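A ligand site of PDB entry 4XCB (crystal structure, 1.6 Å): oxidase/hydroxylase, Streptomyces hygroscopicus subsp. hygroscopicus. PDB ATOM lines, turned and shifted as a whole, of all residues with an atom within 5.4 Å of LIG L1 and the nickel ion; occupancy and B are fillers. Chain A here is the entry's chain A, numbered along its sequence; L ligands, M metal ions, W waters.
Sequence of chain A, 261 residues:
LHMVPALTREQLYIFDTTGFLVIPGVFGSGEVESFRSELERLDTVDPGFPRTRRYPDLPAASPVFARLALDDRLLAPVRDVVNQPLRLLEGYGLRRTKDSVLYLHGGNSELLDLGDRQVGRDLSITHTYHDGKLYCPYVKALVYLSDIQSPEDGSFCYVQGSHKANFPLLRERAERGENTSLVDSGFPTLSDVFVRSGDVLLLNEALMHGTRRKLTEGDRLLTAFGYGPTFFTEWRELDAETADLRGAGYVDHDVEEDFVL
O2 of LIG L1 sits at hydrogen-bond distance from OH of Tyr 92 (2.5 Å).
The side-chain hydroxyl (OH) of Tyr 144 sits at hydrogen-bond distance from an oxygen (O4) of LIG L1.
NH2 of Arg 220 is in salt-bridge range of O4 of LIG L1 (2.8 Å).
O2 of LIG L1 is in salt-bridge range of NZ of Lys 140, 3.97 Å away.
O12 of LG2 L2 is in hydrogen-bond range of NZ of Lys 140.
The side-chain carboxylate (OE1) of Glu 205 lies within salt-bridge range of a nitrogen (N3) of LG2 L2 (3.3 Å).
The side-chain hydroxyl (OH) of Tyr 92 is in hydrogen-bond range of the side-chain amino group (NZ) of Lys 140, at 2.8 Å.
The backbone carbonyl oxygen (O) of Tyr 92 lies within hydrogen-bond range of the backbone NH (N) of Ala 224 (2.8 Å).
The backbone NH of Arg 220 is in hydrogen-bond range of the backbone carbonyl oxygen of Arg 96 (2.8 Å).
NH2 of Arg 220 lies within hydrogen-bond range of O of Gly 154.
The backbone NH of Leu 203 is in hydrogen-bond range of the backbone carbonyl oxygen of Lys 140 (2.8 Å).
The backbone NH (N) of Thr 211 is in hydrogen-bond range of the backbone carbonyl oxygen (O) of Leu 102 (2.9 Å).
The side-chain hydroxyl of Thr 211 lies within hydrogen-bond range of the guanidinium group of Arg 96.
The backbone carbonyl oxygen of Leu 222 lies within hydrogen-bond range of the backbone NH of Leu 94, 3.0 Å away.
Leu 94 touches LIG L1.
CD2 of Leu 102 touches C3 of LIG L1, 3.6 Å away.
CD1 of Leu 142 touches C4 of LIG L1, at 3.9 Å.
Phe 156 touches LIG L1 (CD2 to O4, 3.9 Å).
Thr 211 touches LIG L1.
Leu 222 touches LIG L1 (CD1 to C5, 3.9 Å).
Hydrophobic or aromatic side chains that line LIG L1: Tyr 92, Leu 94, Leu 102, His 105, Leu 142, Tyr 144, Phe 156, His 209 and Leu 222.
Of the 19 residues printed, 12 come within 4 Å of LIG L1.
The nearest printed residue that does not touch LIG L1 is Arg 96 (4.4 Å).
Of the 19 residues printed, 2 come within 4 Å of the nickel ion.
The nickel ion is bound by water W4 (2.0 Å), O1 of LIG L1 (2.0 Å), NE2 of His 209 (2.1 Å), NE2 of His 105 (2.1 Å), O3 of LIG L1 (2.1 Å) and water W1 (2.3 Å).
The nickel ion has six donor atoms within binding distance.
Water W1 bridges the side-chain carboxylate of Glu 205 (2.7 Å) and the side-chain amino group of Lys 140 (3.0 Å).
Water W4 lies within hydrogen-bond range of OE1 of Glu 205, NZ of Lys 140 and O7 of LG2 L2.
Water W3 lies within hydrogen-bond range of an oxygen (O2) of LIG L1 (2.7 Å) and an oxygen (O10) of LG2 L2 (2.8 Å).
Water W2 lies within hydrogen-bond range of an oxygen (O5) of LIG L1 (2.7 Å), the guanidinium group (NH1) of Arg 96 (3.0 Å) and the guanidinium group (NH1) of Arg 220 (3.3 Å).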
ATOM      1  N   TYR A  92      12.571 -28.696  16.434  1.00  0.00           N
ATOM      2  CA  TYR A  92      12.097 -29.051  15.098  1.00  0.00           C
ATOM      3  C   TYR A  92      12.533 -28.041  14.054  1.00  0.00           C
ATOM      4  O   TYR A  92      13.043 -26.972  14.372  1.00  0.00           O
ATOM      5  CB  TYR A  92      10.565 -29.189  15.095  1.00  0.00           C
ATOM      6  CG  TYR A  92       9.819 -27.915  15.454  1.00  0.00           C
ATOM      7  CD1 TYR A  92       9.514 -27.626  16.775  1.00  0.00           C
ATOM      8  CD2 TYR A  92       9.406 -27.040  14.469  1.00  0.00           C
ATOM      9  CE1 TYR A  92       8.833 -26.480  17.112  1.00  0.00           C
ATOM     10  CE2 TYR A  92       8.728 -25.890  14.793  1.00  0.00           C
ATOM     11  CZ  TYR A  92       8.437 -25.620  16.118  1.00  0.00           C
ATOM     12  OH  TYR A  92       7.750 -24.472  16.439  1.00  0.00           O
ATOM     13  N   LEU A  94      11.412 -26.165  10.147  1.00  0.00           N
ATOM     14  CA  LEU A  94      10.327 -25.849   9.215  1.00  0.00           C
ATOM     15  C   LEU A  94      10.893 -25.306   7.920  1.00  0.00           C
ATOM     16  O   LEU A  94      11.625 -24.305   7.923  1.00  0.00           O
ATOM     17  CB  LEU A  94       9.343 -24.850   9.827  1.00  0.00           C
ATOM     18  CG  LEU A  94       8.515 -25.325  11.026  1.00  0.00           C
ATOM     19  CD1 LEU A  94       7.771 -24.129  11.618  1.00  0.00           C
ATOM     20  CD2 LEU A  94       7.534 -26.426  10.599  1.00  0.00           C
ATOM     21  N   ARG A  96       9.580 -23.919   4.230  1.00  0.00           N
ATOM     22  CA  ARG A  96       8.375 -23.463   3.538  1.00  0.00           C
ATOM     23  C   ARG A  96       8.662 -22.893   2.158  1.00  0.00           C
ATOM     24  O   ARG A  96       9.702 -22.279   1.932  1.00  0.00           O
ATOM     25  CB  ARG A  96       7.656 -22.398   4.361  1.00  0.00           C
ATOM     26  CG  ARG A  96       6.839 -22.962   5.512  1.00  0.00           C
ATOM     27  CD  ARG A  96       6.382 -21.855   6.428  1.00  0.00           C
ATOM     28  NE  ARG A  96       5.706 -20.789   5.698  1.00  0.00           N
ATOM     29  CZ  ARG A  96       5.344 -19.630   6.245  1.00  0.00           C
ATOM     30  NH1 ARG A  96       5.585 -19.398   7.523  1.00  0.00           N
ATOM     31  NH2 ARG A  96       4.751 -18.692   5.512  1.00  0.00           N
ATOM     32  N   LEU A 102       1.180 -19.395   8.282  1.00  0.00           N
ATOM     33  CA  LEU A 102       0.983 -19.942   9.627  1.00  0.00           C
ATOM     34  C   LEU A 102       0.040 -19.044  10.394  1.00  0.00           C
ATOM     35  O   LEU A 102       0.387 -17.913  10.749  1.00  0.00           O
ATOM     36  CB  LEU A 102       2.323 -20.090  10.361  1.00  0.00           C
ATOM     37  CG  LEU A 102       2.310 -20.891  11.659  1.00  0.00           C
ATOM     38  CD1 LEU A 102       1.811 -22.287  11.400  1.00  0.00           C
ATOM     39  CD2 LEU A 102       3.707 -20.945  12.233  1.00  0.00           C
ATOM     40  N   HIS A 105      -1.580 -18.210  16.685  1.00  0.00           N
ATOM     41  CA  HIS A 105      -1.708 -19.163  17.798  1.00  0.00           C
ATOM     42  C   HIS A 105      -1.089 -18.540  19.022  1.00  0.00           C
ATOM     43  O   HIS A 105      -0.364 -17.559  18.916  1.00  0.00           O
ATOM     44  CB  HIS A 105      -1.052 -20.506  17.471  1.00  0.00           C
ATOM     45  CG  HIS A 105       0.336 -20.395  16.885  1.00  0.00           C
ATOM     46  ND1 HIS A 105       0.560 -20.139  15.554  1.00  0.00           N
ATOM     47  CD2 HIS A 105       1.549 -20.529  17.459  1.00  0.00           C
ATOM     48  CE1 HIS A 105       1.869 -20.104  15.332  1.00  0.00           C
ATOM     49  NE2 HIS A 105       2.486 -20.346  16.469  1.00  0.00           N
ATOM     50  N   LYS A 140      10.635 -20.339  23.274  1.00  0.00           N
ATOM     51  CA  LYS A 140      11.271 -20.896  22.108  1.00  0.00           C
ATOM     52  C   LYS A 140      12.410 -20.033  21.644  1.00  0.00           C
ATOM     53  O   LYS A 140      12.325 -18.803  21.695  1.00  0.00           O
ATOM     54  CB  LYS A 140      10.273 -21.051  20.968  1.00  0.00           C
ATOM     55  CG  LYS A 140       9.390 -22.235  21.071  1.00  0.00           C
ATOM     56  CD  LYS A 140       8.646 -22.423  19.776  1.00  0.00           C
ATOM     57  CE  LYS A 140       7.602 -23.500  19.919  1.00  0.00           C
ATOM     58  NZ  LYS A 140       6.617 -23.437  18.791  1.00  0.00           N
ATOM     59  N   LEU A 142      13.915 -19.414  18.141  1.00  0.00           N
ATOM     60  CA  LEU A 142      13.829 -19.618  16.711  1.00  0.00           C
ATOM     61  C   LEU A 142      15.130 -19.165  16.065  1.00  0.00           C
ATOM     62  O   LEU A 142      15.479 -17.988  16.121  1.00  0.00           O
ATOM     63  CB  LEU A 142      12.650 -18.850  16.109  1.00  0.00           C
ATOM     64  CG  LEU A 142      11.264 -18.992  16.745  1.00  0.00           C
ATOM     65  CD1 LEU A 142      10.273 -18.075  16.077  1.00  0.00           C
ATOM     66  CD2 LEU A 142      10.771 -20.400  16.622  1.00  0.00           C
ATOM     67  N   TYR A 144      16.697 -18.550  12.681  1.00  0.00           N
ATOM     68  CA  TYR A 144      16.350 -18.407  11.273  1.00  0.00           C
ATOM     69  C   TYR A 144      17.549 -18.698  10.389  1.00  0.00           C
ATOM     70  O   TYR A 144      18.673 -18.285  10.681  1.00  0.00           O
ATOM     71  CB  TYR A 144      15.814 -17.004  10.991  1.00  0.00           C
ATOM     72  CG  TYR A 144      14.423 -16.800  11.539  1.00  0.00           C
ATOM     73  CD1 TYR A 144      14.235 -16.238  12.806  1.00  0.00           C
ATOM     74  CD2 TYR A 144      13.300 -17.186  10.816  1.00  0.00           C
ATOM     75  CE1 TYR A 144      12.966 -16.054  13.316  1.00  0.00           C
ATOM     76  CE2 TYR A 144      12.021 -17.004  11.324  1.00  0.00           C
ATOM     77  CZ  TYR A 144      11.859 -16.446  12.579  1.00  0.00           C
ATOM     78  OH  TYR A 144      10.589 -16.253  13.085  1.00  0.00           O
ATOM     79  N   ILE A 148      14.266 -12.958   5.928  1.00  0.00           N
ATOM     80  CA  ILE A 148      12.853 -12.668   5.824  1.00  0.00           C
ATOM     81  C   ILE A 148      12.701 -11.164   6.016  1.00  0.00           C
ATOM     82  O   ILE A 148      12.714 -10.647   7.136  1.00  0.00           O
ATOM     83  CB  ILE A 148      12.036 -13.485   6.867  1.00  0.00           C
ATOM     84  CG1 ILE A 148      12.335 -14.976   6.749  1.00  0.00           C
ATOM     85  CG2 ILE A 148      10.548 -13.221   6.675  1.00  0.00           C
ATOM     86  CD1 ILE A 148      11.730 -15.834   7.857  1.00  0.00           C
ATOM     87  N   GLY A 154       6.858 -14.005   4.134  1.00  0.00           N
ATOM     88  CA  GLY A 154       6.220 -14.751   5.203  1.00  0.00           C
ATOM     89  C   GLY A 154       6.763 -14.331   6.547  1.00  0.00           C
ATOM     90  O   GLY A 154       7.123 -15.158   7.385  1.00  0.00           O
ATOM     91  N   PHE A 156       7.329 -13.317  10.283  1.00  0.00           N
ATOM     92  CA  PHE A 156       6.760 -13.481  11.604  1.00  0.00           C
ATOM     93  C   PHE A 156       5.866 -12.289  11.908  1.00  0.00           C
ATOM     94  O   PHE A 156       6.203 -11.153  11.559  1.00  0.00           O
ATOM     95  CB  PHE A 156       7.905 -13.597  12.620  1.00  0.00           C
ATOM     96  CG  PHE A 156       7.467 -13.806  14.034  1.00  0.00           C
ATOM     97  CD1 PHE A 156       7.155 -12.723  14.832  1.00  0.00           C
ATOM     98  CD2 PHE A 156       7.415 -15.078  14.565  1.00  0.00           C
ATOM     99  CE1 PHE A 156       6.784 -12.909  16.145  1.00  0.00           C
ATOM    100  CE2 PHE A 156       7.045 -15.273  15.883  1.00  0.00           C
ATOM    101  CZ  PHE A 156       6.726 -14.187  16.665  1.00  0.00           C
ATOM    102  N   LEU A 203      11.220 -16.244  22.125  1.00  0.00           N
ATOM    103  CA  LEU A 203       9.768 -16.058  22.088  1.00  0.00           C
ATOM    104  C   LEU A 203       9.068 -16.602  23.332  1.00  0.00           C
ATOM    105  O   LEU A 203       9.199 -17.767  23.664  1.00  0.00           O
ATOM    106  CB  LEU A 203       9.200 -16.744  20.842  1.00  0.00           C
ATOM    107  CG  LEU A 203       7.693 -16.767  20.633  1.00  0.00           C
ATOM    108  CD1 LEU A 203       7.173 -15.337  20.497  1.00  0.00           C
ATOM    109  CD2 LEU A 203       7.364 -17.562  19.378  1.00  0.00           C
ATOM    110  N   GLU A 205       5.898 -18.060  24.609  1.00  0.00           N
ATOM    111  CA  GLU A 205       4.836 -18.735  23.854  1.00  0.00           C
ATOM    112  C   GLU A 205       3.444 -18.225  24.251  1.00  0.00           C
ATOM    113  O   GLU A 205       2.447 -18.562  23.613  1.00  0.00           O
ATOM    114  CB  GLU A 205       4.944 -20.252  24.012  1.00  0.00           C
ATOM    115  CG  GLU A 205       6.001 -20.848  23.071  1.00  0.00           C
ATOM    116  CD  GLU A 205       5.622 -20.717  21.598  1.00  0.00           C
ATOM    117  OE1 GLU A 205       4.526 -21.183  21.213  1.00  0.00           O
ATOM    118  OE2 GLU A 205       6.412 -20.139  20.827  1.00  0.00           O
ATOM    119  N   HIS A 209       0.899 -15.171  17.927  1.00  0.00           N
ATOM    120  CA  HIS A 209       1.805 -14.935  16.820  1.00  0.00           C
ATOM    121  C   HIS A 209       1.568 -15.929  15.690  1.00  0.00           C
ATOM    122  O   HIS A 209       0.843 -16.906  15.829  1.00  0.00           O
ATOM    123  CB  HIS A 209       3.250 -15.048  17.310  1.00  0.00           C
ATOM    124  CG  HIS A 209       3.603 -16.426  17.767  1.00  0.00           C
ATOM    125  ND1 HIS A 209       3.221 -16.934  18.989  1.00  0.00           N
ATOM    126  CD2 HIS A 209       4.247 -17.424  17.117  1.00  0.00           C
ATOM    127  CE1 HIS A 209       3.648 -18.178  19.088  1.00  0.00           C
ATOM    128  NE2 HIS A 209       4.272 -18.500  17.973  1.00  0.00           N
ATOM    129  N   GLY A 210       2.202 -15.664  14.547  1.00  0.00           N
ATOM    130  CA  GLY A 210       2.112 -16.549  13.412  1.00  0.00           C
ATOM    131  C   GLY A 210       3.008 -15.963  12.341  1.00  0.00           C
ATOM    132  O   GLY A 210       3.961 -15.267  12.648  1.00  0.00           O
ATOM    133  N   THR A 211       2.711 -16.248  11.076  1.00  0.00           N
ATOM    134  CA  THR A 211       3.422 -15.551  10.011  1.00  0.00           C
ATOM    135  C   THR A 211       2.482 -15.158   8.891  1.00  0.00           C
ATOM    136  O   THR A 211       1.426 -15.753   8.719  1.00  0.00           O
ATOM    137  CB  THR A 211       4.553 -16.386   9.393  1.00  0.00           C
ATOM    138  OG1 THR A 211       4.019 -17.238   8.375  1.00  0.00           O
ATOM    139  CG2 THR A 211       5.265 -17.225  10.453  1.00  0.00           C
ATOM    140  N   ARG A 220      11.901 -20.827   2.738  1.00  0.00           N
ATOM    141  CA  ARG A 220      11.929 -20.161   4.028  1.00  0.00           C
ATOM    142  C   ARG A 220      12.275 -21.223   5.049  1.00  0.00           C
ATOM    143  O   ARG A 220      11.636 -22.273   5.092  1.00  0.00           O
ATOM    144  CB  ARG A 220      10.585 -19.494   4.327  1.00  0.00           C
ATOM    145  CG  ARG A 220      10.502 -18.728   5.634  1.00  0.00           C
ATOM    146  CD  ARG A 220       9.025 -18.469   5.961  1.00  0.00           C
ATOM    147  NE  ARG A 220       8.839 -17.469   7.008  1.00  0.00           N
ATOM    148  CZ  ARG A 220       8.850 -17.734   8.306  1.00  0.00           C
ATOM    149  NH1 ARG A 220       9.092 -18.975   8.716  1.00  0.00           N
ATOM    150  NH2 ARG A 220       8.655 -16.759   9.186  1.00  0.00           N
ATOM    151  N   LEU A 222      13.903 -22.401   9.079  1.00  0.00           N
ATOM    152  CA  LEU A 222      14.321 -22.109  10.433  1.00  0.00           C
ATOM    153  C   LEU A 222      14.269 -23.362  11.282  1.00  0.00           C
ATOM    154  O   LEU A 222      13.681 -24.361  10.891  1.00  0.00           O
ATOM    155  CB  LEU A 222      13.440 -21.033  11.073  1.00  0.00           C
ATOM    156  CG  LEU A 222      12.097 -21.495  11.615  1.00  0.00           C
ATOM    157  CD1 LEU A 222      11.465 -20.398  12.446  1.00  0.00           C
ATOM    158  CD2 LEU A 222      11.168 -21.910  10.503  1.00  0.00           C
ATOM    159  N   ALA A 224      13.527 -24.472  15.451  1.00  0.00           N
ATOM    160  CA  ALA A 224      12.933 -23.964  16.691  1.00  0.00           C
ATOM    161  C   ALA A 224      13.238 -24.894  17.833  1.00  0.00           C
ATOM    162  O   ALA A 224      13.097 -26.117  17.716  1.00  0.00           O
ATOM    163  CB  ALA A 224      11.432 -23.831  16.531  1.00  0.00           C
HETATM  164  C1  LIG L   1       5.965 -21.922  15.403  1.00  0.00           C
HETATM  165  O1  LIG L   1       5.170 -22.139  16.370  1.00  0.00           O
HETATM  166  O2  LIG L   1       6.602 -22.881  14.860  1.00  0.00           O
HETATM  167  C2  LIG L   1       6.165 -20.527  14.896  1.00  0.00           C
HETATM  168  O3  LIG L   1       5.621 -19.622  15.522  1.00  0.00           O
HETATM  169  C3  LIG L   1       6.963 -20.273  13.635  1.00  0.00           C
HETATM  170  C4  LIG L   1       7.503 -18.865  13.520  1.00  0.00           C
HETATM  171  C5  LIG L   1       8.038 -18.631  12.120  1.00  0.00           C
HETATM  172  O4  LIG L   1       8.658 -17.553  11.860  1.00  0.00           O
HETATM  173  O5  LIG L   1       7.862 -19.502  11.236  1.00  0.00           O
HETATM  174  C1  LG2 L   2      -3.261 -27.105  17.848  1.00  0.00           C
HETATM  175  C2  LG2 L   2      -4.688 -27.491  17.520  1.00  0.00           C
HETATM  176  C3  LG2 L   2      -4.709 -28.805  16.757  1.00  0.00           C
HETATM  177  C4  LG2 L   2      -3.885 -28.692  15.476  1.00  0.00           C
HETATM  178  C5  LG2 L   2      -2.469 -28.203  15.765  1.00  0.00           C
HETATM  179  C6  LG2 L   2      -2.443 -26.947  16.591  1.00  0.00           C
HETATM  180  N1  LG2 L   2      -5.403 -27.618  18.733  1.00  0.00           N
HETATM  181  O1  LG2 L   2      -3.293 -25.863  18.518  1.00  0.00           O
HETATM  182  N2  LG2 L   2      -3.830 -29.970  14.866  1.00  0.00           N
HETATM  183  C7  LG2 L   2      -5.078 -30.196  14.128  1.00  0.00           C
HETATM  184  O2  LG2 L   2      -1.853 -27.919  14.525  1.00  0.00           O
HETATM  185  C8  LG2 L   2       0.646 -25.051  17.445  1.00  0.00           C
HETATM  186  C9  LG2 L   2      -0.653 -25.355  16.758  1.00  0.00           C
HETATM  187  O3  LG2 L   2      -0.635 -25.116  15.378  1.00  0.00           O
HETATM  188  C10 LG2 L   2      -0.320 -23.779  15.104  1.00  0.00           C
HETATM  189  C11 LG2 L   2       1.140 -23.610  15.368  1.00  0.00           C
HETATM  190  C12 LG2 L   2       1.372 -23.896  16.912  1.00  0.00           C
HETATM  191  O4  LG2 L   2      -1.063 -26.699  16.964  1.00  0.00           O
HETATM  192  C13 LG2 L   2      -0.640 -23.484  13.638  1.00  0.00           C
HETATM  193  O5  LG2 L   2      -2.064 -23.467  13.479  1.00  0.00           O
HETATM  194  O6  LG2 L   2       1.874 -24.503  14.624  1.00  0.00           O
HETATM  195  O7  LG2 L   2       2.703 -24.079  17.111  1.00  0.00           O
HETATM  196  C14 LG2 L   2       2.842 -25.347  17.784  1.00  0.00           C
HETATM  197  C15 LG2 L   2       4.106 -25.998  17.344  1.00  0.00           C
HETATM  198  C16 LG2 L   2       4.440 -27.165  18.266  1.00  0.00           C
HETATM  199  C17 LG2 L   2       4.451 -26.734  19.716  1.00  0.00           C
HETATM  200  C18 LG2 L   2       3.120 -26.157  20.036  1.00  0.00           C
HETATM  201  O8  LG2 L   2       2.885 -25.070  19.164  1.00  0.00           O
HETATM  202  O9  LG2 L   2       1.634 -26.162  17.456  1.00  0.00           O
HETATM  203  O10 LG2 L   2       3.975 -26.541  16.027  1.00  0.00           O
HETATM  204  O11 LG2 L   2       5.681 -27.711  17.863  1.00  0.00           O
HETATM  205  O12 LG2 L   2       5.476 -25.766  19.975  1.00  0.00           O
HETATM  206  C19 LG2 L   2       3.089 -25.621  21.480  1.00  0.00           C
HETATM  207  C20 LG2 L   2       1.656 -25.522  21.954  1.00  0.00           C
HETATM  208  O13 LG2 L   2       1.119 -26.797  22.254  1.00  0.00           O
HETATM  209  N3  LG2 L   2       3.636 -24.325  21.500  1.00  0.00           N
HETATM  210 NI    NI M   1       4.497 -20.415  17.169  1.00  0.00          NI
HETATM  211  O   HOH W   1       6.589 -20.486  18.110  1.00  0.00           O
HETATM  212  O   HOH W   2       6.867 -21.312   9.428  1.00  0.00           O
HETATM  213  O   HOH W   3       4.621 -24.587  14.184  1.00  0.00           O
HETATM  214  O   HOH W   4       4.108 -21.533  18.792  1.00  0.00           O
